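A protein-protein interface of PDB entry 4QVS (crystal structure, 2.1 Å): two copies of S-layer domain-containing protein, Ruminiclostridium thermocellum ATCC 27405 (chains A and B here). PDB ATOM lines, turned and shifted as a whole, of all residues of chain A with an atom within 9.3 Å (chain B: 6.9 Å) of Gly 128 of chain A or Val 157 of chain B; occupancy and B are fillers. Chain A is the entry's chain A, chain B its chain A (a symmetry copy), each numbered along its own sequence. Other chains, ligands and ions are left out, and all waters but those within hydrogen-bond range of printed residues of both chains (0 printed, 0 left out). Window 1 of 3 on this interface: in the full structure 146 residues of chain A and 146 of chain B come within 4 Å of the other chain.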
ATOM      1  N   LEU A 102       6.866 -19.271   9.540  1.00  0.00           N
ATOM      2  CA  LEU A 102       5.467 -19.506   9.107  1.00  0.00           C
ATOM      3  C   LEU A 102       5.412 -18.860   7.756  1.00  0.00           C
ATOM      4  O   LEU A 102       5.876 -17.734   7.599  1.00  0.00           O
ATOM      5  CB  LEU A 102       4.424 -18.875  10.024  1.00  0.00           C
ATOM      6  CG  LEU A 102       2.946 -19.068   9.583  1.00  0.00           C
ATOM      7  CD1 LEU A 102       2.479 -20.480   9.809  1.00  0.00           C
ATOM      8  CD2 LEU A 102       2.056 -18.128  10.359  1.00  0.00           C
ATOM      9  N   GLU A 105       1.535 -19.980   1.355  1.00  0.00           N
ATOM     10  CA  GLU A 105       1.859 -20.899   0.269  1.00  0.00           C
ATOM     11  C   GLU A 105       1.300 -20.492  -1.105  1.00  0.00           C
ATOM     12  O   GLU A 105       0.626 -19.458  -1.241  1.00  0.00           O
ATOM     13  CB  GLU A 105       1.425 -22.310   0.682  1.00  0.00           C
ATOM     14  CG  GLU A 105       2.110 -22.769   1.969  1.00  0.00           C
ATOM     15  CD  GLU A 105       3.614 -22.899   1.796  1.00  0.00           C
ATOM     16  OE1 GLU A 105       4.055 -23.920   1.239  1.00  0.00           O
ATOM     17  OE2 GLU A 105       4.355 -22.002   2.251  1.00  0.00           O
ATOM     18  N   ASP A 107      -1.133 -21.064  -2.709  1.00  0.00           N
ATOM     19  CA  ASP A 107      -2.569 -20.990  -2.911  1.00  0.00           C
ATOM     20  C   ASP A 107      -3.438 -20.447  -1.784  1.00  0.00           C
ATOM     21  O   ASP A 107      -4.669 -20.544  -1.857  1.00  0.00           O
ATOM     22  CB  ASP A 107      -3.016 -22.402  -3.268  1.00  0.00           C
ATOM     23  CG  ASP A 107      -2.262 -23.466  -2.469  1.00  0.00           C
ATOM     24  OD1 ASP A 107      -1.143 -23.193  -1.913  1.00  0.00           O
ATOM     25  OD2 ASP A 107      -2.793 -24.590  -2.423  1.00  0.00           O
ATOM     26  N   GLY A 108      -2.845 -19.833  -0.769  1.00  0.00           N
ATOM     27  CA  GLY A 108      -3.652 -19.307   0.353  1.00  0.00           C
ATOM     28  C   GLY A 108      -3.503 -20.206   1.565  1.00  0.00           C
ATOM     29  O   GLY A 108      -3.877 -19.826   2.678  1.00  0.00           O
ATOM     30  N   LYS A 109      -2.991 -21.421   1.360  1.00  0.00           N
ATOM     31  CA  LYS A 109      -2.643 -22.258   2.497  1.00  0.00           C
ATOM     32  C   LYS A 109      -1.488 -21.561   3.232  1.00  0.00           C
ATOM     33  O   LYS A 109      -0.964 -20.551   2.748  1.00  0.00           O
ATOM     34  CB  LYS A 109      -2.165 -23.628   2.066  1.00  0.00           C
ATOM     35  CG  LYS A 109      -3.191 -24.410   1.295  1.00  0.00           C
ATOM     36  CD  LYS A 109      -2.751 -25.839   1.086  1.00  0.00           C
ATOM     37  CE  LYS A 109      -1.534 -25.959   0.205  1.00  0.00           C
ATOM     38  NZ  LYS A 109      -1.524 -27.299  -0.437  1.00  0.00           N
ATOM     39  N   ILE A 110      -1.178 -22.069   4.421  1.00  0.00           N
ATOM     40  CA  ILE A 110      -0.078 -21.576   5.246  1.00  0.00           C
ATOM     41  C   ILE A 110       0.697 -22.789   5.720  1.00  0.00           C
ATOM     42  O   ILE A 110       0.138 -23.884   5.830  1.00  0.00           O
ATOM     43  CB  ILE A 110      -0.510 -20.736   6.482  1.00  0.00           C
ATOM     44  CG1 ILE A 110      -1.402 -21.531   7.424  1.00  0.00           C
ATOM     45  CG2 ILE A 110      -1.191 -19.457   6.049  1.00  0.00           C
ATOM     46  CD1 ILE A 110      -1.963 -20.752   8.608  1.00  0.00           C
ATOM     47  N   LYS A 111       1.983 -22.588   5.962  1.00  0.00           N
ATOM     48  CA  LYS A 111       2.844 -23.653   6.427  1.00  0.00           C
ATOM     49  C   LYS A 111       3.742 -23.172   7.539  1.00  0.00           C
ATOM     50  O   LYS A 111       4.297 -22.075   7.498  1.00  0.00           O
ATOM     51  CB  LYS A 111       3.746 -24.141   5.306  1.00  0.00           C
ATOM     52  CG  LYS A 111       4.630 -25.314   5.708  1.00  0.00           C
ATOM     53  CD  LYS A 111       5.309 -25.927   4.502  1.00  0.00           C
ATOM     54  CE  LYS A 111       6.430 -25.007   4.024  1.00  0.00           C
ATOM     55  NZ  LYS A 111       6.881 -25.332   2.646  1.00  0.00           N
ATOM     56  N   ILE A 125       3.960 -28.244   9.116  1.00  0.00           N
ATOM     57  CA  ILE A 125       2.513 -28.403   9.269  1.00  0.00           C
ATOM     58  C   ILE A 125       1.940 -27.520   8.190  1.00  0.00           C
ATOM     59  O   ILE A 125       2.318 -26.346   8.088  1.00  0.00           O
ATOM     60  CB  ILE A 125       1.958 -27.853  10.581  1.00  0.00           C
ATOM     61  CG1 ILE A 125       2.901 -28.115  11.745  1.00  0.00           C
ATOM     62  CG2 ILE A 125       0.574 -28.437  10.834  1.00  0.00           C
ATOM     63  CD1 ILE A 125       2.517 -27.360  13.001  1.00  0.00           C
ATOM     64  N   THR A 126       1.024 -28.055   7.391  1.00  0.00           N
ATOM     65  CA  THR A 126       0.443 -27.292   6.290  1.00  0.00           C
ATOM     66  C   THR A 126      -1.070 -27.284   6.385  1.00  0.00           C
ATOM     67  O   THR A 126      -1.663 -28.307   6.641  1.00  0.00           O
ATOM     68  CB  THR A 126       0.859 -27.896   4.938  1.00  0.00           C
ATOM     69  OG1 THR A 126       2.282 -28.046   4.902  1.00  0.00           O
ATOM     70  CG2 THR A 126       0.423 -26.998   3.807  1.00  0.00           C
ATOM     71  N   SER A 127      -1.704 -26.137   6.166  1.00  0.00           N
ATOM     72  CA  SER A 127      -3.172 -26.076   6.225  1.00  0.00           C
ATOM     73  C   SER A 127      -3.852 -26.823   5.047  1.00  0.00           C
ATOM     74  O   SER A 127      -3.198 -27.161   4.054  1.00  0.00           O
ATOM     75  CB  SER A 127      -3.645 -24.629   6.320  1.00  0.00           C
ATOM     76  OG  SER A 127      -3.251 -23.855   5.209  1.00  0.00           O
ATOM     77  N   GLY A 128      -5.155 -27.092   5.174  1.00  0.00           N
ATOM     78  CA  GLY A 128      -5.922 -27.881   4.171  1.00  0.00           C
ATOM     79  C   GLY A 128      -6.238 -27.223   2.834  1.00  0.00           C
ATOM     80  O   GLY A 128      -6.298 -26.006   2.733  1.00  0.00           O
ATOM     81  N   SER A 129      -6.424 -28.029   1.789  1.00  0.00           N
ATOM     82  CA  SER A 129      -6.806 -27.502   0.471  1.00  0.00           C
ATOM     83  C   SER A 129      -8.310 -27.132   0.527  1.00  0.00           C
ATOM     84  O   SER A 129      -9.012 -27.524   1.459  1.00  0.00           O
ATOM     85  CB  SER A 129      -6.576 -28.532  -0.651  1.00  0.00           C
ATOM     86  OG  SER A 129      -5.416 -29.306  -0.433  1.00  0.00           O
ATOM     87  N   ALA A 130      -8.745 -26.379  -0.486  1.00  0.00           N
ATOM     88  CA  ALA A 130     -10.117 -25.892  -0.687  1.00  0.00           C
ATOM     89  C   ALA A 130     -10.329 -25.869  -2.217  1.00  0.00           C
ATOM     90  O   ALA A 130      -9.356 -26.079  -2.958  1.00  0.00           O
ATOM     91  CB  ALA A 130     -10.269 -24.494  -0.106  1.00  0.00           C
ATOM     92  N   LEU A 131     -11.552 -25.612  -2.696  1.00  0.00           N
ATOM     93  CA  LEU A 131     -11.791 -25.537  -4.157  1.00  0.00           C
ATOM     94  C   LEU A 131     -11.592 -24.145  -4.683  1.00  0.00           C
ATOM     95  O   LEU A 131     -12.299 -23.233  -4.278  1.00  0.00           O
ATOM     96  CB  LEU A 131     -13.216 -25.956  -4.543  1.00  0.00           C
ATOM     97  CG  LEU A 131     -13.561 -27.416  -4.534  1.00  0.00           C
ATOM     98  CD1 LEU A 131     -15.064 -27.575  -4.893  1.00  0.00           C
ATOM     99  CD2 LEU A 131     -12.672 -28.141  -5.532  1.00  0.00           C
ATOM    100  N   THR A 132     -10.687 -24.014  -5.650  1.00  0.00           N
ATOM    101  CA  THR A 132     -10.278 -22.724  -6.211  1.00  0.00           C
ATOM    102  C   THR A 132     -11.004 -22.488  -7.502  1.00  0.00           C
ATOM    103  O   THR A 132     -11.199 -23.425  -8.266  1.00  0.00           O
ATOM    104  CB  THR A 132      -8.770 -22.723  -6.524  1.00  0.00           C
ATOM    105  OG1 THR A 132      -8.055 -23.128  -5.358  1.00  0.00           O
ATOM    106  CG2 THR A 132      -8.293 -21.345  -6.986  1.00  0.00           C
ATOM    107  N   LYS A 137     -10.302 -29.942  -9.668  1.00  0.00           N
ATOM    108  CA  LYS A 137      -9.827 -30.669  -8.485  1.00  0.00           C
ATOM    109  C   LYS A 137     -10.623 -31.975  -8.339  1.00  0.00           C
ATOM    110  O   LYS A 137     -11.708 -32.086  -8.887  1.00  0.00           O
ATOM    111  CB  LYS A 137      -9.929 -29.794  -7.223  1.00  0.00           C
ATOM    112  CG  LYS A 137      -8.857 -28.697  -7.116  1.00  0.00           C
ATOM    113  CD  LYS A 137      -8.838 -28.055  -5.727  1.00  0.00           C
ATOM    114  CE  LYS A 137      -7.532 -27.299  -5.425  1.00  0.00           C
ATOM    115  NZ  LYS A 137      -7.452 -26.076  -6.250  1.00  0.00           N
ATOM    116  N   ILE A 152      -9.965 -33.829  -0.957  1.00  0.00           N
ATOM    117  CA  ILE A 152      -9.724 -32.946  -2.097  1.00  0.00           C
ATOM    118  C   ILE A 152      -8.382 -33.404  -2.661  1.00  0.00           C
ATOM    119  O   ILE A 152      -7.431 -33.536  -1.919  1.00  0.00           O
ATOM    120  CB  ILE A 152      -9.643 -31.471  -1.718  1.00  0.00           C
ATOM    121  CG1 ILE A 152     -11.010 -30.992  -1.215  1.00  0.00           C
ATOM    122  CG2 ILE A 152      -9.218 -30.663  -2.942  1.00  0.00           C
ATOM    123  CD1 ILE A 152     -11.036 -29.554  -0.750  1.00  0.00           C
ATOM    124  N   GLU A 155      -6.374 -35.849  -0.486  1.00  0.00           N
ATOM    125  CA  GLU A 155      -5.954 -35.405   0.825  1.00  0.00           C
ATOM    126  C   GLU A 155      -7.166 -35.282   1.714  1.00  0.00           C
ATOM    127  O   GLU A 155      -8.172 -34.711   1.324  1.00  0.00           O
ATOM    128  CB  GLU A 155      -5.262 -34.046   0.727  1.00  0.00           C
ATOM    129  CG  GLU A 155      -5.297 -33.226   2.015  1.00  0.00           C
ATOM    130  CD  GLU A 155      -4.784 -31.809   1.818  1.00  0.00           C
ATOM    131  OE1 GLU A 155      -3.804 -31.629   1.061  1.00  0.00           O
ATOM    132  OE2 GLU A 155      -5.350 -30.874   2.423  1.00  0.00           O
ATOM    133  N   ASN A 156      -7.044 -35.805   2.924  1.00  0.00           N
ATOM    134  CA  ASN A 156      -8.100 -35.756   3.926  1.00  0.00           C
ATOM    135  C   ASN A 156      -8.258 -34.349   4.475  1.00  0.00           C
ATOM    136  O   ASN A 156      -7.311 -33.781   5.060  1.00  0.00           O
ATOM    137  CB  ASN A 156      -7.797 -36.752   5.051  1.00  0.00           C
ATOM    138  CG  ASN A 156      -8.762 -36.633   6.206  1.00  0.00           C
ATOM    139  OD1 ASN A 156      -9.530 -35.684   6.266  1.00  0.00           O
ATOM    140  ND2 ASN A 156      -8.728 -37.602   7.133  1.00  0.00           N
ATOM    141  N   VAL A 157      -9.460 -33.798   4.316  1.00  0.00           N
ATOM    142  CA  VAL A 157      -9.763 -32.411   4.716  1.00  0.00           C
ATOM    143  C   VAL A 157     -10.917 -32.241   5.741  1.00  0.00           C
ATOM    144  O   VAL A 157     -11.369 -31.128   5.998  1.00  0.00           O
ATOM    145  CB  VAL A 157     -10.012 -31.538   3.457  1.00  0.00           C
ATOM    146  CG1 VAL A 157      -8.721 -31.398   2.645  1.00  0.00           C
ATOM    147  CG2 VAL A 157     -11.137 -32.121   2.589  1.00  0.00           C
ATOM    148  N   GLY A 158     -11.372 -33.344   6.331  1.00  0.00           N
ATOM    149  CA  GLY A 158     -12.432 -33.319   7.332  1.00  0.00           C
ATOM    150  C   GLY A 158     -12.946 -34.726   7.600  1.00  0.00           C
ATOM    151  O   GLY A 158     -12.880 -35.584   6.723  1.00  0.00           O
ATOM    152  N   GLY B 128     -11.560 -27.470   5.585  1.00  0.00           N
ATOM    153  CA  GLY B 128     -10.824 -26.416   6.337  1.00  0.00           C
ATOM    154  C   GLY B 128     -10.754 -25.021   5.728  1.00  0.00           C
ATOM    155  O   GLY B 128     -10.859 -24.857   4.522  1.00  0.00           O
ATOM    156  N   SER B 129     -10.594 -23.999   6.569  1.00  0.00           N
ATOM    157  CA  SER B 129     -10.440 -22.621   6.082  1.00  0.00           C
ATOM    158  C   SER B 129      -8.998 -22.470   5.533  1.00  0.00           C
ATOM    159  O   SER B 129      -8.147 -23.324   5.781  1.00  0.00           O
ATOM    160  CB  SER B 129     -10.671 -21.584   7.198  1.00  0.00           C
ATOM    161  OG  SER B 129     -11.690 -21.982   8.089  1.00  0.00           O
ATOM    162  N   ALA B 130      -8.784 -21.378   4.797  1.00  0.00           N
ATOM    163  CA  ALA B 130      -7.518 -20.985   4.163  1.00  0.00           C
ATOM    164  C   ALA B 130      -7.493 -19.441   4.209  1.00  0.00           C
ATOM    165  O   ALA B 130      -8.513 -18.838   4.577  1.00  0.00           O
ATOM    166  CB  ALA B 130      -7.474 -21.477   2.725  1.00  0.00           C
ATOM    167  N   ALA B 140      -2.844 -18.589  14.248  1.00  0.00           N
ATOM    168  CA  ALA B 140      -2.059 -18.968  15.420  1.00  0.00           C
ATOM    169  C   ALA B 140      -1.366 -20.297  15.191  1.00  0.00           C
ATOM    170  O   ALA B 140      -1.847 -21.123  14.416  1.00  0.00           O
ATOM    171  CB  ALA B 140      -2.935 -19.040  16.657  1.00  0.00           C
ATOM    172  N   THR B 149       0.193 -27.139  16.358  1.00  0.00           N
ATOM    173  CA  THR B 149      -1.122 -26.919  15.735  1.00  0.00           C
ATOM    174  C   THR B 149      -1.297 -25.564  15.045  1.00  0.00           C
ATOM    175  O   THR B 149      -0.908 -24.519  15.570  1.00  0.00           O
ATOM    176  CB  THR B 149      -2.227 -27.091  16.796  1.00  0.00           C
ATOM    177  OG1 THR B 149      -2.073 -28.370  17.417  1.00  0.00           O
ATOM    178  CG2 THR B 149      -3.628 -26.991  16.176  1.00  0.00           C
ATOM    179  N   LEU B 150      -1.879 -25.598  13.855  1.00  0.00           N
ATOM    180  CA  LEU B 150      -2.205 -24.399  13.110  1.00  0.00           C
ATOM    181  C   LEU B 150      -3.651 -24.100  13.283  1.00  0.00           C
ATOM    182  O   LEU B 150      -4.503 -25.009  13.178  1.00  0.00           O
ATOM    183  CB  LEU B 150      -1.997 -24.598  11.623  1.00  0.00           C
ATOM    184  CG  LEU B 150      -0.574 -24.518  11.132  1.00  0.00           C
ATOM    185  CD1 LEU B 150      -0.473 -24.954   9.673  1.00  0.00           C
ATOM    186  CD2 LEU B 150      -0.086 -23.092  11.325  1.00  0.00           C
ATOM    187  N   TYR B 151      -3.932 -22.817  13.468  1.00  0.00           N
ATOM    188  CA  TYR B 151      -5.279 -22.319  13.598  1.00  0.00           C
ATOM    189  C   TYR B 151      -5.527 -21.115  12.696  1.00  0.00           C
ATOM    190  O   TYR B 151      -4.674 -20.211  12.599  1.00  0.00           O
ATOM    191  CB  TYR B 151      -5.539 -21.810  15.008  1.00  0.00           C
ATOM    192  CG  TYR B 151      -5.502 -22.817  16.107  1.00  0.00           C
ATOM    193  CD1 TYR B 151      -4.314 -23.134  16.765  1.00  0.00           C
ATOM    194  CD2 TYR B 151      -6.677 -23.388  16.559  1.00  0.00           C
ATOM    195  CE1 TYR B 151      -4.297 -24.041  17.805  1.00  0.00           C
ATOM    196  CE2 TYR B 151      -6.670 -24.298  17.579  1.00  0.00           C
ATOM    197  CZ  TYR B 151      -5.498 -24.622  18.200  1.00  0.00           C
ATOM    198  OH  TYR B 151      -5.574 -25.509  19.224  1.00  0.00           O
ATOM    199  N   ILE B 152      -6.706 -21.100  12.064  1.00  0.00           N
ATOM    200  CA  ILE B 152      -7.189 -19.960  11.287  1.00  0.00           C
ATOM    201  C   ILE B 152      -8.520 -19.590  11.934  1.00  0.00           C
ATOM    202  O   ILE B 152      -9.352 -20.450  12.133  1.00  0.00           O
ATOM    203  CB  ILE B 152      -7.408 -20.278   9.812  1.00  0.00           C
ATOM    204  CG1 ILE B 152      -6.062 -20.583   9.144  1.00  0.00           C
ATOM    205  CG2 ILE B 152      -8.074 -19.082   9.136  1.00  0.00           C
ATOM    206  CD1 ILE B 152      -6.162 -20.975   7.688  1.00  0.00           C
ATOM    207  N   GLU B 155      -9.934 -22.109  14.463  1.00  0.00           N
ATOM    208  CA  GLU B 155     -10.248 -23.441  13.994  1.00  0.00           C
ATOM    209  C   GLU B 155      -8.964 -24.164  13.674  1.00  0.00           C
ATOM    210  O   GLU B 155      -8.090 -23.626  13.012  1.00  0.00           O
ATOM    211  CB  GLU B 155     -11.112 -23.368  12.735  1.00  0.00           C
ATOM    212  CG  GLU B 155     -11.027 -24.603  11.840  1.00  0.00           C
ATOM    213  CD  GLU B 155     -11.733 -24.406  10.508  1.00  0.00           C
ATOM    214  OE1 GLU B 155     -12.810 -23.771  10.492  1.00  0.00           O
ATOM    215  OE2 GLU B 155     -11.220 -24.893   9.477  1.00  0.00           O
ATOM    216  N   ASN B 156      -8.875 -25.403  14.132  1.00  0.00           N
ATOM    217  CA  ASN B 156      -7.722 -26.262  13.898  1.00  0.00           C
ATOM    218  C   ASN B 156      -7.677 -26.721  12.451  1.00  0.00           C
ATOM    219  O   ASN B 156      -8.612 -27.393  11.965  1.00  0.00           O
ATOM    220  CB  ASN B 156      -7.762 -27.460  14.852  1.00  0.00           C
ATOM    221  CG  ASN B 156      -6.690 -28.478  14.550  1.00  0.00           C
ATOM    222  OD1 ASN B 156      -6.045 -28.398  13.514  1.00  0.00           O
ATOM    223  ND2 ASN B 156      -6.492 -29.446  15.457  1.00  0.00           N
ATOM    224  N   VAL B 157      -6.582 -26.388  11.773  1.00  0.00           N
ATOM    225  CA  VAL B 157      -6.409 -26.683  10.337  1.00  0.00           C
ATOM    226  C   VAL B 157      -5.172 -27.546   9.970  1.00  0.00           C
ATOM    227  O   VAL B 157      -4.836 -27.694   8.797  1.00  0.00           O
ATOM    228  CB  VAL B 157      -6.422 -25.364   9.520  1.00  0.00           C
ATOM    229  CG1 VAL B 157      -7.808 -24.715   9.583  1.00  0.00           C
ATOM    230  CG2 VAL B 157      -5.344 -24.389  10.016  1.00  0.00           C
ATOM    231  N   GLY B 158      -4.516 -28.124  10.972  1.00  0.00           N
ATOM    232  CA  GLY B 158      -3.356 -28.982  10.761  1.00  0.00           C
ATOM    233  C   GLY B 158      -2.642 -29.248  12.079  1.00  0.00           C
ATOM    234  O   GLY B 158      -2.703 -28.427  12.990  1.00  0.00           O
ATOM    235  N   GLU B 159      -1.996 -30.414  12.170  1.00  0.00           N
ATOM    236  CA  GLU B 159      -1.196 -30.855  13.323  1.00  0.00           C
ATOM    237  C   GLU B 159      -0.048 -31.746  12.870  1.00  0.00           C
ATOM    238  O   GLU B 159      -0.088 -32.373  11.809  1.00  0.00           O
ATOM    239  CB  GLU B 159      -1.987 -31.730  14.298  1.00  0.00           C
ATOM    240  CG  GLU B 159      -2.971 -31.064  15.222  1.00  0.00           C
ATOM    241  CD  GLU B 159      -3.753 -32.118  15.991  1.00  0.00           C
ATOM    242  OE1 GLU B 159      -3.160 -33.138  16.407  1.00  0.00           O
ATOM    243  OE2 GLU B 159      -4.968 -31.941  16.152  1.00  0.00           O
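N of Ile 110 of chain A sits at hydrogen-bond distance from OG of Ser 127 of chain A, 2.8 Å away. The backbone NH (N) of Val 157 of chain B sits at hydrogen-bond distance from the backbone carbonyl oxygen (O) of Leu 150 of chain B (2.9 Å). N of Leu 150 of chain B is in hydrogen-bond range of O of Gly 158 of chain B (3.1 Å). OD1 of Asn 156 of chain B sits at hydrogen-bond distance from N of Gly 158 of chain B (3.0 Å). ND2 of Asn 156 of chain B is in hydrogen-bond range of OE2 of Glu 159 of chain B (3.0 Å).
Gly 128 of chain A touches Val 157 of chain B, and with the chains exchanged Val 157 of chain A touches Gly 128 of chain B.
Leu 102 of chain A touches Leu 150 of chain B (CD1 to CD2, 3.96 Å). Gly 108 of chain A touches Ala 130 of chain B. Leu 150 of chain B touches Ile 125 of chain A (CD1 to O, 3.5 Å). Ile 125 of chain A touches Gly 158 of chain B (CG2 to C, 3.5 Å). Ile 125 of chain A touches Glu 159 of chain B (CG2 to N, 3.5 Å). O of Thr 126 of chain A touches O of Val 157 of chain B, 3.9 Å away. CD1 of Leu 150 of chain B touches N of Ser 127 of chain A, 3.9 Å away. CA of Ser 127 of chain A touches O of Val 157 of chain B, at 3.5 Å. Gly 128 of chain A touches Val 157 of chain B. Val 157 of chain A touches Gly 128 of chain B (O to N, 3.7 Å).
Printed residues of chain B that touch a printed residue of chain A: Gly 128, Ala 130, Leu 150, Val 157, Gly 158 and Glu 159. Hydrophobic or aromatic side chains of chain B that line the printed part of chain A: Ala 130 and Leu 150. Of the 21 printed residues of chain A, 7 touch a printed residue of chain B. Along chain A the printed residues that touch a printed residue of chain B span positions 102 to 157.
Printed residues of chain B within 4 Å of Ile 125 of chain A: Leu 150 (3.5 Å), Gly 158 (3.5 Å) and Glu 159 (3.5 Å). Gly 128 of chain A touches just one residue of chain B: Val 157 (3.7 Å). Of the printed residues of chain B, Val 157 of chain A touches Gly 128 (3.7 Å). Printed residues of chain A within 4 Å of Gly 128 of chain B: Val 157. Val 157 of chain B touches just these residues of chain A: Thr 126, Ser 127 and Gly 128. Gly 158 of chain B touches just one residue of chain A: Ile 125. Printed residues of chain A within 4 Å of Glu 159 of chain B: Ile 125 (3.5 Å). The nearest printed residue of chain B that does not touch Ser 127 of chain A is Ile 152 of chain B (4.6 Å).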
